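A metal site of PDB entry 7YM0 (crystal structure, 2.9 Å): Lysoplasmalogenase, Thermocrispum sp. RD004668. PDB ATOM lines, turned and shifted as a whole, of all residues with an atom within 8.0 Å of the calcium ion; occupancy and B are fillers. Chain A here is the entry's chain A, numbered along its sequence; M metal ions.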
ATOM      1  N   HIS A  20      24.219  31.802   1.502  1.00  0.00           N
ATOM      2  CA  HIS A  20      24.349  30.838   0.408  1.00  0.00           C
ATOM      3  C   HIS A  20      25.436  31.289  -0.550  1.00  0.00           C
ATOM      4  O   HIS A  20      25.248  32.259  -1.294  1.00  0.00           O
ATOM      5  CB  HIS A  20      23.007  30.680  -0.296  1.00  0.00           C
ATOM      6  CG  HIS A  20      22.977  29.568  -1.306  1.00  0.00           C
ATOM      7  ND1 HIS A  20      23.117  29.786  -2.658  1.00  0.00           N
ATOM      8  CD2 HIS A  20      22.821  28.233  -1.153  1.00  0.00           C
ATOM      9  CE1 HIS A  20      23.058  28.633  -3.302  1.00  0.00           C
ATOM     10  NE2 HIS A  20      22.869  27.674  -2.404  1.00  0.00           N
ATOM     11  N   ALA A  21      26.579  30.603  -0.527  1.00  0.00           N
ATOM     12  CA  ALA A  21      27.772  31.003  -1.304  1.00  0.00           C
ATOM     13  C   ALA A  21      28.192  32.425  -0.952  1.00  0.00           C
ATOM     14  O   ALA A  21      28.751  33.143  -1.787  1.00  0.00           O
ATOM     15  CB  ALA A  21      27.559  30.854  -2.811  1.00  0.00           C
ATOM     16  N   GLU A  24      24.730  34.870  -3.186  1.00  0.00           N
ATOM     17  CA  GLU A  24      25.053  34.914  -4.614  1.00  0.00           C
ATOM     18  C   GLU A  24      24.320  36.018  -5.350  1.00  0.00           C
ATOM     19  O   GLU A  24      24.735  36.385  -6.462  1.00  0.00           O
ATOM     20  CB  GLU A  24      24.717  33.565  -5.259  1.00  0.00           C
ATOM     21  CG  GLU A  24      23.379  32.989  -4.814  1.00  0.00           C
ATOM     22  CD  GLU A  24      23.127  31.599  -5.312  1.00  0.00           C
ATOM     23  OE1 GLU A  24      24.109  30.915  -5.724  1.00  0.00           O
ATOM     24  OE2 GLU A  24      21.946  31.176  -5.300  1.00  0.00           O
ATOM     25  N   ASN A  30      30.870  32.818  -3.762  1.00  0.00           N
ATOM     26  CA  ASN A  30      32.069  32.064  -3.396  1.00  0.00           C
ATOM     27  C   ASN A  30      33.342  32.882  -3.544  1.00  0.00           C
ATOM     28  O   ASN A  30      34.335  32.434  -4.119  1.00  0.00           O
ATOM     29  CB  ASN A  30      32.168  30.749  -4.181  1.00  0.00           C
ATOM     30  CG  ASN A  30      31.203  29.701  -3.676  1.00  0.00           C
ATOM     31  OD1 ASN A  30      31.073  29.485  -2.476  1.00  0.00           O
ATOM     32  ND2 ASN A  30      30.516  29.045  -4.595  1.00  0.00           N
ATOM     33  N   GLU A  47      27.854  29.228   3.870  1.00  0.00           N
ATOM     34  CA  GLU A  47      27.660  28.075   2.992  1.00  0.00           C
ATOM     35  C   GLU A  47      28.540  28.238   1.746  1.00  0.00           C
ATOM     36  O   GLU A  47      28.502  29.281   1.093  1.00  0.00           O
ATOM     37  CB  GLU A  47      26.190  27.941   2.571  1.00  0.00           C
ATOM     38  CG  GLU A  47      25.837  26.611   1.901  1.00  0.00           C
ATOM     39  CD  GLU A  47      26.003  26.642   0.387  1.00  0.00           C
ATOM     40  OE1 GLU A  47      26.166  27.755  -0.168  1.00  0.00           O
ATOM     41  OE2 GLU A  47      25.964  25.552  -0.245  1.00  0.00           O
ATOM     42  N   LEU A  48      29.320  27.198   1.427  1.00  0.00           N
ATOM     43  CA  LEU A  48      30.163  27.271   0.233  1.00  0.00           C
ATOM     44  C   LEU A  48      30.259  25.896  -0.426  1.00  0.00           C
ATOM     45  O   LEU A  48      29.798  24.888   0.117  1.00  0.00           O
ATOM     46  CB  LEU A  48      31.569  27.819   0.555  1.00  0.00           C
ATOM     47  CG  LEU A  48      32.288  27.322   1.823  1.00  0.00           C
ATOM     48  CD1 LEU A  48      32.888  25.948   1.598  1.00  0.00           C
ATOM     49  CD2 LEU A  48      33.373  28.317   2.239  1.00  0.00           C
ATOM     50  N   ASP A  49      30.855  25.887  -1.614  1.00  0.00           N
ATOM     51  CA  ASP A  49      31.035  24.707  -2.442  1.00  0.00           C
ATOM     52  C   ASP A  49      32.520  24.577  -2.788  1.00  0.00           C
ATOM     53  O   ASP A  49      33.209  25.577  -2.967  1.00  0.00           O
ATOM     54  CB  ASP A  49      30.180  24.785  -3.731  1.00  0.00           C
ATOM     55  CG  ASP A  49      28.782  25.388  -3.483  1.00  0.00           C
ATOM     56  OD1 ASP A  49      27.872  24.672  -3.006  1.00  0.00           O
ATOM     57  OD2 ASP A  49      28.595  26.590  -3.784  1.00  0.00           O
ATOM     58  N   VAL A  50      33.014  23.342  -2.866  1.00  0.00           N
ATOM     59  CA  VAL A  50      34.441  23.114  -3.093  1.00  0.00           C
ATOM     60  C   VAL A  50      34.648  22.166  -4.273  1.00  0.00           C
ATOM     61  O   VAL A  50      33.908  21.195  -4.441  1.00  0.00           O
ATOM     62  CB  VAL A  50      35.160  22.587  -1.836  1.00  0.00           C
ATOM     63  CG1 VAL A  50      34.928  23.513  -0.666  1.00  0.00           C
ATOM     64  CG2 VAL A  50      34.679  21.178  -1.499  1.00  0.00           C
ATOM     65  N   ILE A  61      34.172  27.119  -5.245  1.00  0.00           N
ATOM     66  CA  ILE A  61      33.501  27.381  -6.517  1.00  0.00           C
ATOM     67  C   ILE A  61      32.460  26.284  -6.731  1.00  0.00           C
ATOM     68  O   ILE A  61      32.687  25.125  -6.383  1.00  0.00           O
ATOM     69  CB  ILE A  61      34.504  27.442  -7.693  1.00  0.00           C
ATOM     70  CG1 ILE A  61      33.779  27.440  -9.041  1.00  0.00           C
ATOM     71  CG2 ILE A  61      35.462  26.267  -7.655  1.00  0.00           C
ATOM     72  CD1 ILE A  61      34.691  27.745 -10.247  1.00  0.00           C
ATOM     73  N   HIS A  62      31.307  26.654  -7.282  1.00  0.00           N
ATOM     74  CA  HIS A  62      30.155  25.745  -7.345  1.00  0.00           C
ATOM     75  C   HIS A  62      30.208  24.862  -8.579  1.00  0.00           C
ATOM     76  O   HIS A  62      30.223  23.634  -8.481  1.00  0.00           O
ATOM     77  CB  HIS A  62      28.864  26.570  -7.323  1.00  0.00           C
ATOM     78  CG  HIS A  62      27.616  25.758  -7.493  1.00  0.00           C
ATOM     79  ND1 HIS A  62      27.126  25.383  -8.730  1.00  0.00           N
ATOM     80  CD2 HIS A  62      26.738  25.287  -6.577  1.00  0.00           C
ATOM     81  CE1 HIS A  62      26.015  24.684  -8.563  1.00  0.00           C
ATOM     82  NE2 HIS A  62      25.751  24.616  -7.269  1.00  0.00           N
ATOM     83  N   ASN A 147      29.557  25.757   6.307  1.00  0.00           N
ATOM     84  CA  ASN A 147      28.822  24.646   5.716  1.00  0.00           C
ATOM     85  C   ASN A 147      29.465  24.351   4.376  1.00  0.00           C
ATOM     86  O   ASN A 147      29.517  25.231   3.495  1.00  0.00           O
ATOM     87  CB  ASN A 147      27.344  25.006   5.563  1.00  0.00           C
ATOM     88  CG  ASN A 147      26.443  23.786   5.489  1.00  0.00           C
ATOM     89  OD1 ASN A 147      25.852  23.375   6.490  1.00  0.00           O
ATOM     90  ND2 ASN A 147      26.303  23.220   4.292  1.00  0.00           N
ATOM     91  N   ILE A 148      29.989  23.126   4.204  1.00  0.00           N
ATOM     92  CA  ILE A 148      30.832  22.812   3.064  1.00  0.00           C
ATOM     93  C   ILE A 148      30.195  21.678   2.263  1.00  0.00           C
ATOM     94  O   ILE A 148      29.980  20.582   2.789  1.00  0.00           O
ATOM     95  CB  ILE A 148      32.259  22.444   3.505  1.00  0.00           C
ATOM     96  CG1 ILE A 148      32.846  23.556   4.378  1.00  0.00           C
ATOM     97  CG2 ILE A 148      33.134  22.189   2.292  1.00  0.00           C
ATOM     98  CD1 ILE A 148      34.054  23.145   5.172  1.00  0.00           C
ATOM     99  N   GLU A 149      29.902  21.947   0.994  1.00  0.00           N
ATOM    100  CA  GLU A 149      29.310  20.978   0.090  1.00  0.00           C
ATOM    101  C   GLU A 149      30.384  20.477  -0.867  1.00  0.00           C
ATOM    102  O   GLU A 149      31.096  21.269  -1.478  1.00  0.00           O
ATOM    103  CB  GLU A 149      28.145  21.576  -0.692  1.00  0.00           C
ATOM    104  CG  GLU A 149      27.343  20.541  -1.473  1.00  0.00           C
ATOM    105  CD  GLU A 149      26.357  21.155  -2.451  1.00  0.00           C
ATOM    106  OE1 GLU A 149      26.076  20.520  -3.506  1.00  0.00           O
ATOM    107  OE2 GLU A 149      25.867  22.277  -2.184  1.00  0.00           O
ATOM    108  N   ILE A 150      30.480  19.144  -0.995  1.00  0.00           N
ATOM    109  CA  ILE A 150      31.441  18.512  -1.882  1.00  0.00           C
ATOM    110  C   ILE A 150      30.831  18.417  -3.280  1.00  0.00           C
ATOM    111  O   ILE A 150      29.734  17.876  -3.448  1.00  0.00           O
ATOM    112  CB  ILE A 150      31.841  17.120  -1.367  1.00  0.00           C
ATOM    113  CG1 ILE A 150      32.303  17.214   0.075  1.00  0.00           C
ATOM    114  CG2 ILE A 150      32.926  16.504  -2.252  1.00  0.00           C
ATOM    115  CD1 ILE A 150      32.665  15.881   0.689  1.00  0.00           C
ATOM    116  N   LYS A 151      31.549  18.934  -4.268  1.00  0.00           N
ATOM    117  CA  LYS A 151      31.101  18.948  -5.650  1.00  0.00           C
ATOM    118  C   LYS A 151      31.974  18.029  -6.492  1.00  0.00           C
ATOM    119  O   LYS A 151      33.059  17.611  -6.085  1.00  0.00           O
ATOM    120  CB  LYS A 151      31.120  20.376  -6.205  1.00  0.00           C
ATOM    121  CG  LYS A 151      30.255  21.331  -5.423  1.00  0.00           C
ATOM    122  CD  LYS A 151      28.773  21.015  -5.601  1.00  0.00           C
ATOM    123  CE  LYS A 151      27.906  22.273  -5.507  1.00  0.00           C
ATOM    124  NZ  LYS A 151      26.495  21.999  -5.859  1.00  0.00           N
ATOM    125  N   THR A 183      28.647  18.080   3.593  1.00  0.00           N
ATOM    126  CA  THR A 183      27.602  17.365   2.863  1.00  0.00           C
ATOM    127  C   THR A 183      28.000  17.311   1.395  1.00  0.00           C
ATOM    128  O   THR A 183      29.129  17.663   1.025  1.00  0.00           O
ATOM    129  CB  THR A 183      26.236  18.033   3.105  1.00  0.00           C
ATOM    130  OG1 THR A 183      25.193  17.280   2.477  1.00  0.00           O
ATOM    131  CG2 THR A 183      26.214  19.457   2.537  1.00  0.00           C
ATOM    132  N   PHE A 185      25.691  16.247  -2.673  1.00  0.00           N
ATOM    133  CA  PHE A 185      24.558  15.539  -3.242  1.00  0.00           C
ATOM    134  C   PHE A 185      24.818  14.045  -3.368  1.00  0.00           C
ATOM    135  O   PHE A 185      23.865  13.266  -3.490  1.00  0.00           O
ATOM    136  CB  PHE A 185      24.186  16.127  -4.604  1.00  0.00           C
ATOM    137  CG  PHE A 185      23.366  17.371  -4.512  1.00  0.00           C
ATOM    138  CD1 PHE A 185      22.516  17.579  -3.437  1.00  0.00           C
ATOM    139  CD2 PHE A 185      23.450  18.363  -5.489  1.00  0.00           C
ATOM    140  CE1 PHE A 185      21.762  18.729  -3.336  1.00  0.00           C
ATOM    141  CE2 PHE A 185      22.690  19.524  -5.396  1.00  0.00           C
ATOM    142  CZ  PHE A 185      21.845  19.702  -4.324  1.00  0.00           C
ATOM    143  N   GLN A 227      19.427  19.095   5.263  1.00  0.00           N
ATOM    144  CA  GLN A 227      19.472  20.313   4.455  1.00  0.00           C
ATOM    145  C   GLN A 227      18.674  20.052   3.190  1.00  0.00           C
ATOM    146  O   GLN A 227      19.076  19.246   2.337  1.00  0.00           O
ATOM    147  CB  GLN A 227      20.914  20.738   4.179  1.00  0.00           C
ATOM    148  CG  GLN A 227      21.795  20.556   5.420  1.00  0.00           C
ATOM    149  CD  GLN A 227      23.069  21.376   5.384  1.00  0.00           C
ATOM    150  OE1 GLN A 227      23.818  21.341   4.409  1.00  0.00           O
ATOM    151  NE2 GLN A 227      23.307  22.146   6.462  1.00  0.00           N
ATOM    152  N   TRP A 256      17.292  25.514   1.853  1.00  0.00           N
ATOM    153  CA  TRP A 256      17.865  26.341   0.796  1.00  0.00           C
ATOM    154  C   TRP A 256      16.836  26.535  -0.310  1.00  0.00           C
ATOM    155  O   TRP A 256      15.743  25.951  -0.289  1.00  0.00           O
ATOM    156  CB  TRP A 256      19.159  25.727   0.241  1.00  0.00           C
ATOM    157  CG  TRP A 256      19.076  24.279  -0.132  1.00  0.00           C
ATOM    158  CD1 TRP A 256      19.220  23.204   0.713  1.00  0.00           C
ATOM    159  CD2 TRP A 256      18.876  23.743  -1.433  1.00  0.00           C
ATOM    160  NE1 TRP A 256      19.100  22.028   0.011  1.00  0.00           N
ATOM    161  CE2 TRP A 256      18.888  22.330  -1.312  1.00  0.00           C
ATOM    162  CE3 TRP A 256      18.672  24.305  -2.702  1.00  0.00           C
ATOM    163  CZ2 TRP A 256      18.713  21.489  -2.402  1.00  0.00           C
ATOM    164  CZ3 TRP A 256      18.506  23.464  -3.774  1.00  0.00           C
ATOM    165  CH2 TRP A 256      18.529  22.071  -3.625  1.00  0.00           C
ATOM    166  N   SER A 258      17.494  28.415  -4.269  1.00  0.00           N
ATOM    167  CA  SER A 258      18.230  28.186  -5.521  1.00  0.00           C
ATOM    168  C   SER A 258      17.348  27.548  -6.609  1.00  0.00           C
ATOM    169  O   SER A 258      17.680  26.521  -7.188  1.00  0.00           O
ATOM    170  CB  SER A 258      19.481  27.333  -5.239  1.00  0.00           C
ATOM    171  OG  SER A 258      20.050  26.857  -6.450  1.00  0.00           O
ATOM    172  N   MET A 280      19.106  29.385   4.005  1.00  0.00           N
ATOM    173  CA  MET A 280      20.275  29.606   3.150  1.00  0.00           C
ATOM    174  C   MET A 280      19.911  30.592   2.036  1.00  0.00           C
ATOM    175  O   MET A 280      19.658  30.179   0.888  1.00  0.00           O
ATOM    176  CB  MET A 280      20.791  28.300   2.550  1.00  0.00           C
ATOM    177  CG  MET A 280      21.061  27.219   3.566  1.00  0.00           C
ATOM    178  SD  MET A 280      22.063  25.879   2.901  1.00  0.00           S
ATOM    179  CE  MET A 280      21.862  24.686   4.200  1.00  0.00           C
HETATM  180 CA    CA M   1      26.083  24.666  -2.283  1.00  0.00          CA
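Of the 21 residues printed, 3 come within 4 Å of the calcium ion. The nearest printed residue that does not touch the calcium ion is His 62 (4.4 Å).
The side-chain amide nitrogen (ND2) of Asn 30 sits at hydrogen-bond distance from the side-chain carboxylate (OD2) of Asp 49. NZ of Lys 151 is in salt-bridge range of OE1 of Glu 149, at 2.8 Å. N of Ala 21 is in hydrogen-bond range of O of Glu 47 (2.8 Å). The backbone carbonyl oxygen (O) of Leu 48 lies within hydrogen-bond range of the backbone NH (N) of Glu 149 (3.1 Å). The backbone NH of Val 50 sits at hydrogen-bond distance from the backbone carbonyl oxygen of Glu 149 (3.1 Å). The backbone carbonyl oxygen (O) of Asp 49 lies within hydrogen-bond range of the backbone NH (N) of Ile 61 (2.9 Å).
The calcium ion is bound by the side-chain carboxylate (OD1) of Asp 49, 1.9 Å away. OE2 of Glu 47 binds the calcium ion (2.2 Å). OE2 of Glu 149 is bound to the calcium ion (2.4 Å). The calcium ion has three donor atoms within binding distance.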
